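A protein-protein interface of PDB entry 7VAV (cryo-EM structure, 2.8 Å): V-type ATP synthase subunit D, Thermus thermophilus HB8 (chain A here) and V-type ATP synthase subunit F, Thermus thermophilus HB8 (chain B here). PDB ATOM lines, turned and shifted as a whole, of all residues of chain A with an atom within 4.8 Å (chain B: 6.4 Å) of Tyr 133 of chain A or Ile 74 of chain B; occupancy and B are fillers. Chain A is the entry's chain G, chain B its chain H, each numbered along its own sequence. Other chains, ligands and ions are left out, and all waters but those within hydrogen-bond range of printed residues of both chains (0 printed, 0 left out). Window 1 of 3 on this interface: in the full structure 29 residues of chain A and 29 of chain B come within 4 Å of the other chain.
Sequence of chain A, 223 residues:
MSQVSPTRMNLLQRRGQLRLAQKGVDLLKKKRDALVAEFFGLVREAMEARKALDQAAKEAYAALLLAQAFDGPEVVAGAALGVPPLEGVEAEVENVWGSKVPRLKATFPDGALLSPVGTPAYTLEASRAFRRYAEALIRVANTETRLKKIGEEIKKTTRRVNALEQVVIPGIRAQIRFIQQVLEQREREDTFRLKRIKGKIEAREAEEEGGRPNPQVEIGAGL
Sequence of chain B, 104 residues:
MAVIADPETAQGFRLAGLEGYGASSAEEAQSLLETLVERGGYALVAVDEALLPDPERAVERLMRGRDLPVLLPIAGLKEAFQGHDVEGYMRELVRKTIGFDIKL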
ATOM      1  N   ARG A  50     -18.326   9.887 -13.027  1.00  0.00           N
ATOM      2  CA  ARG A  50     -18.671   9.895 -14.445  1.00  0.00           C
ATOM      3  C   ARG A  50     -19.707   8.827 -14.767  1.00  0.00           C
ATOM      4  O   ARG A  50     -20.634   9.068 -15.548  1.00  0.00           O
ATOM      5  CB  ARG A  50     -17.415   9.695 -15.290  1.00  0.00           C
ATOM      6  CG  ARG A  50     -16.623  10.966 -15.543  1.00  0.00           C
ATOM      7  CD  ARG A  50     -17.209  11.767 -16.693  1.00  0.00           C
ATOM      8  NE  ARG A  50     -16.485  13.014 -16.909  1.00  0.00           N
ATOM      9  CZ  ARG A  50     -16.739  13.867 -17.892  1.00  0.00           C
ATOM     10  NH1 ARG A  50     -17.700  13.642 -18.773  1.00  0.00           N
ATOM     11  NH2 ARG A  50     -16.010  14.975 -17.994  1.00  0.00           N
ATOM     12  N   LEU A  53     -23.029  10.052 -13.493  1.00  0.00           N
ATOM     13  CA  LEU A  53     -23.528  11.101 -14.374  1.00  0.00           C
ATOM     14  C   LEU A  53     -24.083  10.524 -15.667  1.00  0.00           C
ATOM     15  O   LEU A  53     -25.107  10.993 -16.173  1.00  0.00           O
ATOM     16  CB  LEU A  53     -22.418  12.103 -14.679  1.00  0.00           C
ATOM     17  CG  LEU A  53     -22.790  13.191 -15.685  1.00  0.00           C
ATOM     18  CD1 LEU A  53     -23.880  14.076 -15.114  1.00  0.00           C
ATOM     19  CD2 LEU A  53     -21.573  14.008 -16.082  1.00  0.00           C
ATOM     20  N   ALA A  56     -27.468   9.051 -14.923  1.00  0.00           N
ATOM     21  CA  ALA A  56     -28.448  10.119 -14.753  1.00  0.00           C
ATOM     22  C   ALA A  56     -28.830  10.737 -16.093  1.00  0.00           C
ATOM     23  O   ALA A  56     -30.003  11.036 -16.336  1.00  0.00           O
ATOM     24  CB  ALA A  56     -27.905  11.186 -13.803  1.00  0.00           C
ATOM     25  N   ALA A  57     -27.850  10.934 -16.976  1.00  0.00           N
ATOM     26  CA  ALA A  57     -28.133  11.494 -18.294  1.00  0.00           C
ATOM     27  C   ALA A  57     -29.025  10.565 -19.105  1.00  0.00           C
ATOM     28  O   ALA A  57     -29.954  11.014 -19.787  1.00  0.00           O
ATOM     29  CB  ALA A  57     -26.827  11.770 -19.038  1.00  0.00           C
ATOM     30  N   ALA A  60     -32.517  10.714 -17.721  1.00  0.00           N
ATOM     31  CA  ALA A  60     -33.109  12.006 -18.049  1.00  0.00           C
ATOM     32  C   ALA A  60     -33.554  12.062 -19.505  1.00  0.00           C
ATOM     33  O   ALA A  60     -34.628  12.590 -19.812  1.00  0.00           O
ATOM     34  CB  ALA A  60     -32.116  13.126 -17.746  1.00  0.00           C
ATOM     35  N   ALA A 129     -35.712  14.880 -13.644  1.00  0.00           N
ATOM     36  CA  ALA A 129     -34.578  14.079 -14.084  1.00  0.00           C
ATOM     37  C   ALA A 129     -33.427  14.967 -14.528  1.00  0.00           C
ATOM     38  O   ALA A 129     -32.260  14.657 -14.273  1.00  0.00           O
ATOM     39  CB  ALA A 129     -35.005  13.139 -15.210  1.00  0.00           C
ATOM     40  N   PHE A 130     -33.738  16.083 -15.190  1.00  0.00           N
ATOM     41  CA  PHE A 130     -32.696  17.027 -15.581  1.00  0.00           C
ATOM     42  C   PHE A 130     -32.024  17.667 -14.373  1.00  0.00           C
ATOM     43  O   PHE A 130     -30.809  17.883 -14.388  1.00  0.00           O
ATOM     44  CB  PHE A 130     -33.280  18.098 -16.496  1.00  0.00           C
ATOM     45  CG  PHE A 130     -33.575  17.608 -17.879  1.00  0.00           C
ATOM     46  CD1 PHE A 130     -33.006  16.435 -18.341  1.00  0.00           C
ATOM     47  CD2 PHE A 130     -34.423  18.311 -18.715  1.00  0.00           C
ATOM     48  CE1 PHE A 130     -33.270  15.974 -19.610  1.00  0.00           C
ATOM     49  CE2 PHE A 130     -34.692  17.852 -19.985  1.00  0.00           C
ATOM     50  CZ  PHE A 130     -34.113  16.683 -20.431  1.00  0.00           C
ATOM     51  N   ARG A 131     -32.790  17.990 -13.330  1.00  0.00           N
ATOM     52  CA  ARG A 131     -32.181  18.548 -12.127  1.00  0.00           C
ATOM     53  C   ARG A 131     -31.274  17.534 -11.437  1.00  0.00           C
ATOM     54  O   ARG A 131     -30.183  17.887 -10.974  1.00  0.00           O
ATOM     55  CB  ARG A 131     -33.262  19.065 -11.177  1.00  0.00           C
ATOM     56  CG  ARG A 131     -33.905  20.359 -11.658  1.00  0.00           C
ATOM     57  CD  ARG A 131     -34.811  20.980 -10.609  1.00  0.00           C
ATOM     58  NE  ARG A 131     -36.010  20.186 -10.370  1.00  0.00           N
ATOM     59  CZ  ARG A 131     -37.150  20.343 -11.029  1.00  0.00           C
ATOM     60  NH1 ARG A 131     -37.279  21.256 -11.978  1.00  0.00           N
ATOM     61  NH2 ARG A 131     -38.188  19.572 -10.723  1.00  0.00           N
ATOM     62  N   ARG A 132     -31.694  16.267 -11.372  1.00  0.00           N
ATOM     63  CA  ARG A 132     -30.810  15.239 -10.822  1.00  0.00           C
ATOM     64  C   ARG A 132     -29.566  15.059 -11.690  1.00  0.00           C
ATOM     65  O   ARG A 132     -28.456  14.853 -11.176  1.00  0.00           O
ATOM     66  CB  ARG A 132     -31.561  13.916 -10.673  1.00  0.00           C
ATOM     67  CG  ARG A 132     -32.791  14.003  -9.787  1.00  0.00           C
ATOM     68  CD  ARG A 132     -33.406  12.636  -9.544  1.00  0.00           C
ATOM     69  NE  ARG A 132     -33.755  11.951 -10.783  1.00  0.00           N
ATOM     70  CZ  ARG A 132     -34.969  11.943 -11.317  1.00  0.00           C
ATOM     71  NH1 ARG A 132     -35.974  12.597 -10.758  1.00  0.00           N
ATOM     72  NH2 ARG A 132     -35.179  11.261 -12.439  1.00  0.00           N
ATOM     73  N   TYR A 133     -29.739  15.135 -13.008  1.00  0.00           N
ATOM     74  CA  TYR A 133     -28.619  15.041 -13.936  1.00  0.00           C
ATOM     75  C   TYR A 133     -27.621  16.171 -13.706  1.00  0.00           C
ATOM     76  O   TYR A 133     -26.406  15.951 -13.700  1.00  0.00           O
ATOM     77  CB  TYR A 133     -29.166  15.048 -15.365  1.00  0.00           C
ATOM     78  CG  TYR A 133     -28.179  15.383 -16.454  1.00  0.00           C
ATOM     79  CD1 TYR A 133     -27.038  14.623 -16.647  1.00  0.00           C
ATOM     80  CD2 TYR A 133     -28.406  16.455 -17.304  1.00  0.00           C
ATOM     81  CE1 TYR A 133     -26.142  14.930 -17.653  1.00  0.00           C
ATOM     82  CE2 TYR A 133     -27.520  16.768 -18.309  1.00  0.00           C
ATOM     83  CZ  TYR A 133     -26.389  16.004 -18.479  1.00  0.00           C
ATOM     84  OH  TYR A 133     -25.506  16.319 -19.482  1.00  0.00           O
ATOM     85  N   ALA A 134     -28.120  17.390 -13.490  1.00  0.00           N
ATOM     86  CA  ALA A 134     -27.235  18.516 -13.202  1.00  0.00           C
ATOM     87  C   ALA A 134     -26.581  18.372 -11.830  1.00  0.00           C
ATOM     88  O   ALA A 134     -25.438  18.807 -11.629  1.00  0.00           O
ATOM     89  CB  ALA A 134     -28.010  19.829 -13.291  1.00  0.00           C
ATOM     90  N   GLU A 135     -27.294  17.775 -10.872  1.00  0.00           N
ATOM     91  CA  GLU A 135     -26.706  17.516  -9.561  1.00  0.00           C
ATOM     92  C   GLU A 135     -25.527  16.559  -9.673  1.00  0.00           C
ATOM     93  O   GLU A 135     -24.515  16.719  -8.980  1.00  0.00           O
ATOM     94  CB  GLU A 135     -27.768  16.959  -8.612  1.00  0.00           C
ATOM     95  CG  GLU A 135     -27.285  16.742  -7.187  1.00  0.00           C
ATOM     96  CD  GLU A 135     -26.996  18.043  -6.462  1.00  0.00           C
ATOM     97  OE1 GLU A 135     -27.614  19.071  -6.809  1.00  0.00           O
ATOM     98  OE2 GLU A 135     -26.150  18.036  -5.542  1.00  0.00           O
ATOM     99  N   ALA A 136     -25.648  15.540 -10.525  1.00  0.00           N
ATOM    100  CA  ALA A 136     -24.496  14.684 -10.801  1.00  0.00           C
ATOM    101  C   ALA A 136     -23.418  15.430 -11.582  1.00  0.00           C
ATOM    102  O   ALA A 136     -22.218  15.201 -11.367  1.00  0.00           O
ATOM    103  CB  ALA A 136     -24.939  13.435 -11.564  1.00  0.00           C
ATOM    104  N   LEU A 137     -23.829  16.321 -12.488  1.00  0.00           N
ATOM    105  CA  LEU A 137     -22.883  17.048 -13.326  1.00  0.00           C
ATOM    106  C   LEU A 137     -21.972  17.944 -12.498  1.00  0.00           C
ATOM    107  O   LEU A 137     -20.775  18.058 -12.786  1.00  0.00           O
ATOM    108  CB  LEU A 137     -23.644  17.872 -14.365  1.00  0.00           C
ATOM    109  CG  LEU A 137     -22.840  18.576 -15.459  1.00  0.00           C
ATOM    110  CD1 LEU A 137     -22.247  17.567 -16.425  1.00  0.00           C
ATOM    111  CD2 LEU A 137     -23.715  19.575 -16.199  1.00  0.00           C
ATOM    112  N   VAL B   3     -25.812  25.529 -22.175  1.00  0.00           N
ATOM    113  CA  VAL B   3     -25.317  24.279 -22.737  1.00  0.00           C
ATOM    114  C   VAL B   3     -25.455  24.332 -24.250  1.00  0.00           C
ATOM    115  O   VAL B   3     -26.510  24.703 -24.776  1.00  0.00           O
ATOM    116  CB  VAL B   3     -26.066  23.055 -22.170  1.00  0.00           C
ATOM    117  CG1 VAL B   3     -25.478  21.775 -22.743  1.00  0.00           C
ATOM    118  CG2 VAL B   3     -25.999  23.045 -20.652  1.00  0.00           C
ATOM    119  N   ILE B   4     -24.386  23.959 -24.949  1.00  0.00           N
ATOM    120  CA  ILE B   4     -24.353  23.944 -26.407  1.00  0.00           C
ATOM    121  C   ILE B   4     -24.418  22.493 -26.863  1.00  0.00           C
ATOM    122  O   ILE B   4     -23.518  21.699 -26.562  1.00  0.00           O
ATOM    123  CB  ILE B   4     -23.098  24.643 -26.949  1.00  0.00           C
ATOM    124  CG1 ILE B   4     -23.114  26.127 -26.575  1.00  0.00           C
ATOM    125  CG2 ILE B   4     -23.002  24.473 -28.454  1.00  0.00           C
ATOM    126  CD1 ILE B   4     -21.789  26.825 -26.788  1.00  0.00           C
ATOM    127  N   PHE B  13     -32.873  21.281 -22.305  1.00  0.00           N
ATOM    128  CA  PHE B  13     -32.148  22.135 -21.370  1.00  0.00           C
ATOM    129  C   PHE B  13     -32.928  23.407 -21.054  1.00  0.00           C
ATOM    130  O   PHE B  13     -32.894  23.896 -19.919  1.00  0.00           O
ATOM    131  CB  PHE B  13     -30.757  22.456 -21.916  1.00  0.00           C
ATOM    132  CG  PHE B  13     -29.718  21.445 -21.526  1.00  0.00           C
ATOM    133  CD1 PHE B  13     -29.394  21.251 -20.193  1.00  0.00           C
ATOM    134  CD2 PHE B  13     -29.085  20.671 -22.483  1.00  0.00           C
ATOM    135  CE1 PHE B  13     -28.446  20.317 -19.822  1.00  0.00           C
ATOM    136  CE2 PHE B  13     -28.138  19.731 -22.115  1.00  0.00           C
ATOM    137  CZ  PHE B  13     -27.817  19.557 -20.784  1.00  0.00           C
ATOM    138  N   ALA B  46     -21.668  23.569 -20.489  1.00  0.00           N
ATOM    139  CA  ALA B  46     -21.548  22.241 -21.068  1.00  0.00           C
ATOM    140  C   ALA B  46     -21.629  22.303 -22.590  1.00  0.00           C
ATOM    141  O   ALA B  46     -22.424  23.050 -23.163  1.00  0.00           O
ATOM    142  CB  ALA B  46     -22.634  21.315 -20.523  1.00  0.00           C
ATOM    143  N   VAL B  47     -20.784  21.507 -23.241  1.00  0.00           N
ATOM    144  CA  VAL B  47     -20.731  21.422 -24.695  1.00  0.00           C
ATOM    145  C   VAL B  47     -20.782  19.954 -25.091  1.00  0.00           C
ATOM    146  O   VAL B  47     -20.140  19.109 -24.456  1.00  0.00           O
ATOM    147  CB  VAL B  47     -19.463  22.095 -25.267  1.00  0.00           C
ATOM    148  CG1 VAL B  47     -19.464  22.037 -26.787  1.00  0.00           C
ATOM    149  CG2 VAL B  47     -19.358  23.537 -24.789  1.00  0.00           C
ATOM    150  N   ASP B  48     -21.560  19.649 -26.129  1.00  0.00           N
ATOM    151  CA  ASP B  48     -21.663  18.278 -26.612  1.00  0.00           C
ATOM    152  C   ASP B  48     -20.290  17.762 -27.028  1.00  0.00           C
ATOM    153  O   ASP B  48     -19.551  18.439 -27.749  1.00  0.00           O
ATOM    154  CB  ASP B  48     -22.640  18.204 -27.785  1.00  0.00           C
ATOM    155  CG  ASP B  48     -23.017  16.780 -28.141  1.00  0.00           C
ATOM    156  OD1 ASP B  48     -22.735  15.868 -27.335  1.00  0.00           O
ATOM    157  OD2 ASP B  48     -23.598  16.572 -29.228  1.00  0.00           O
ATOM    158  N   GLU B  49     -19.951  16.555 -26.566  1.00  0.00           N
ATOM    159  CA  GLU B  49     -18.612  16.025 -26.803  1.00  0.00           C
ATOM    160  C   GLU B  49     -18.374  15.712 -28.276  1.00  0.00           C
ATOM    161  O   GLU B  49     -17.266  15.927 -28.781  1.00  0.00           O
ATOM    162  CB  GLU B  49     -18.374  14.785 -25.936  1.00  0.00           C
ATOM    163  CG  GLU B  49     -19.309  13.615 -26.203  1.00  0.00           C
ATOM    164  CD  GLU B  49     -18.778  12.681 -27.272  1.00  0.00           C
ATOM    165  OE1 GLU B  49     -17.565  12.744 -27.566  1.00  0.00           O
ATOM    166  OE2 GLU B  49     -19.568  11.885 -27.817  1.00  0.00           O
ATOM    167  N   ALA B  50     -19.390  15.207 -28.979  1.00  0.00           N
ATOM    168  CA  ALA B  50     -19.236  14.913 -30.399  1.00  0.00           C
ATOM    169  C   ALA B  50     -19.176  16.178 -31.243  1.00  0.00           C
ATOM    170  O   ALA B  50     -18.750  16.117 -32.401  1.00  0.00           O
ATOM    171  CB  ALA B  50     -20.377  14.017 -30.881  1.00  0.00           C
ATOM    172  N   LEU B  72     -16.760  21.056 -19.529  1.00  0.00           N
ATOM    173  CA  LEU B  72     -16.535  19.623 -19.613  1.00  0.00           C
ATOM    174  C   LEU B  72     -17.342  19.063 -20.773  1.00  0.00           C
ATOM    175  O   LEU B  72     -18.423  19.575 -21.086  1.00  0.00           O
ATOM    176  CB  LEU B  72     -16.927  18.901 -18.312  1.00  0.00           C
ATOM    177  CG  LEU B  72     -18.410  18.726 -17.969  1.00  0.00           C
ATOM    178  CD1 LEU B  72     -18.572  17.679 -16.879  1.00  0.00           C
ATOM    179  CD2 LEU B  72     -19.050  20.040 -17.538  1.00  0.00           C
ATOM    180  N   PRO B  73     -16.841  18.023 -21.433  1.00  0.00           N
ATOM    181  CA  PRO B  73     -17.606  17.399 -22.515  1.00  0.00           C
ATOM    182  C   PRO B  73     -18.700  16.490 -21.978  1.00  0.00           C
ATOM    183  O   PRO B  73     -18.605  15.936 -20.880  1.00  0.00           O
ATOM    184  CB  PRO B  73     -16.544  16.597 -23.276  1.00  0.00           C
ATOM    185  CG  PRO B  73     -15.548  16.238 -22.229  1.00  0.00           C
ATOM    186  CD  PRO B  73     -15.526  17.384 -21.244  1.00  0.00           C
ATOM    187  N   ILE B  74     -19.756  16.344 -22.778  1.00  0.00           N
ATOM    188  CA  ILE B  74     -20.900  15.523 -22.405  1.00  0.00           C
ATOM    189  C   ILE B  74     -21.601  15.066 -23.677  1.00  0.00           C
ATOM    190  O   ILE B  74     -21.546  15.733 -24.713  1.00  0.00           O
ATOM    191  CB  ILE B  74     -21.865  16.289 -21.466  1.00  0.00           C
ATOM    192  CG1 ILE B  74     -22.871  15.328 -20.830  1.00  0.00           C
ATOM    193  CG2 ILE B  74     -22.577  17.406 -22.215  1.00  0.00           C
ATOM    194  CD1 ILE B  74     -22.231  14.159 -20.114  1.00  0.00           C
ATOM    195  N   ALA B  75     -22.246  13.905 -23.597  1.00  0.00           N
ATOM    196  CA  ALA B  75     -22.963  13.362 -24.740  1.00  0.00           C
ATOM    197  C   ALA B  75     -24.275  14.106 -24.968  1.00  0.00           C
ATOM    198  O   ALA B  75     -24.922  14.578 -24.029  1.00  0.00           O
ATOM    199  CB  ALA B  75     -23.241  11.873 -24.536  1.00  0.00           C
ATOM    200  N   GLY B  76     -24.665  14.205 -26.235  1.00  0.00           N
ATOM    201  CA  GLY B  76     -25.920  14.820 -26.606  1.00  0.00           C
ATOM    202  C   GLY B  76     -27.082  13.858 -26.454  1.00  0.00           C
ATOM    203  O   GLY B  76     -26.987  12.807 -25.821  1.00  0.00           O
ATOM    204  N   GLU B  79     -26.339  10.974 -28.971  1.00  0.00           N
ATOM    205  CA  GLU B  79     -25.049  10.404 -28.596  1.00  0.00           C
ATOM    206  C   GLU B  79     -25.146   9.602 -27.303  1.00  0.00           C
ATOM    207  O   GLU B  79     -24.511   8.549 -27.172  1.00  0.00           O
ATOM    208  CB  GLU B  79     -24.006  11.514 -28.466  1.00  0.00           C
ATOM    209  CG  GLU B  79     -22.624  11.024 -28.072  1.00  0.00           C
ATOM    210  CD  GLU B  79     -22.018  10.085 -29.100  1.00  0.00           C
ATOM    211  OE1 GLU B  79     -22.298  10.256 -30.304  1.00  0.00           O
ATOM    212  OE2 GLU B  79     -21.262   9.174 -28.702  1.00  0.00           O
ATOM    213  N   HIS B  84     -21.376   5.002 -24.263  1.00  0.00           N
ATOM    214  CA  HIS B  84     -20.338   6.012 -24.118  1.00  0.00           C
ATOM    215  C   HIS B  84     -19.171   5.419 -23.341  1.00  0.00           C
ATOM    216  O   HIS B  84     -19.351   4.926 -22.223  1.00  0.00           O
ATOM    217  CB  HIS B  84     -20.878   7.255 -23.404  1.00  0.00           C
ATOM    218  CG  HIS B  84     -20.192   8.525 -23.798  1.00  0.00           C
ATOM    219  ND1 HIS B  84     -18.889   8.808 -23.448  1.00  0.00           N
ATOM    220  CD2 HIS B  84     -20.628   9.588 -24.514  1.00  0.00           C
ATOM    221  CE1 HIS B  84     -18.552   9.992 -23.930  1.00  0.00           C
ATOM    222  NE2 HIS B  84     -19.590  10.486 -24.581  1.00  0.00           N
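N of Glu 49 of chain B lies within hydrogen-bond range of O of Ile 74 of chain B (2.6 Å). N of Ile 74 of chain B sits at hydrogen-bond distance from O of Val 47 of chain B (3.3 Å).
The backbone carbonyl oxygen (O) of Pro 73 of chain B lies within hydrogen-bond range of the guanidinium group (NH1) of Arg 50 of chain A, 3.2 Å away.
Of the printed residues of chain B, Arg 50 of chain A touches Leu 72 (3.9 Å) and Pro 73 (3.2 Å). Of the printed residues of chain B, Leu 137 of chain A touches Leu 72 (3.7 Å). Of the printed residues of chain A, Phe 13 of chain B touches Tyr 133 (3.7 Å). Val 47 of chain B touches none of the printed residues of chain A. Printed residues of chain A within 4 Å of Leu 72 of chain B: Arg 50 (3.9 Å) and Leu 137 (3.7 Å). Printed residues of chain A within 4 Å of Pro 73 of chain B: Arg 50. Of chain A, only Tyr 133 (3.1 Å) comes within 4 Å of Ile 74 of chain B. The nearest printed residue of chain A that does not touch Pro 73 of chain B is Leu 53 of chain A (6.0 Å).
Printed residues of chain A that touch a printed residue of chain B: Arg 50, Tyr 133 and Leu 137. Hydrophobic or aromatic side chains of chain A within 4 Å of the printed part of chain B: Tyr 133 and Leu 137. Of the 15 printed residues of chain B, 4 touch a printed residue of chain A. Hydrophobic or aromatic side chains of chain B that line the printed part of chain A: Phe 13, Leu 72 and Ile 74. Among the printed residues, no Asp or Glu carboxylate lies within 4 Å of a Lys or Arg side-chain nitrogen of the other chain.
Among the printed residues, merely in contact across the chains: Tyr 133 of chain A with Ile 74 of chain B (3.1 Å), Leu 137 of chain A with Leu 72 of chain B (3.7 Å), Tyr 133 of chain A with Phe 13 of chain B (3.7 Å) and Arg 50 of chain A with Leu 72 of chain B (3.9 Å).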
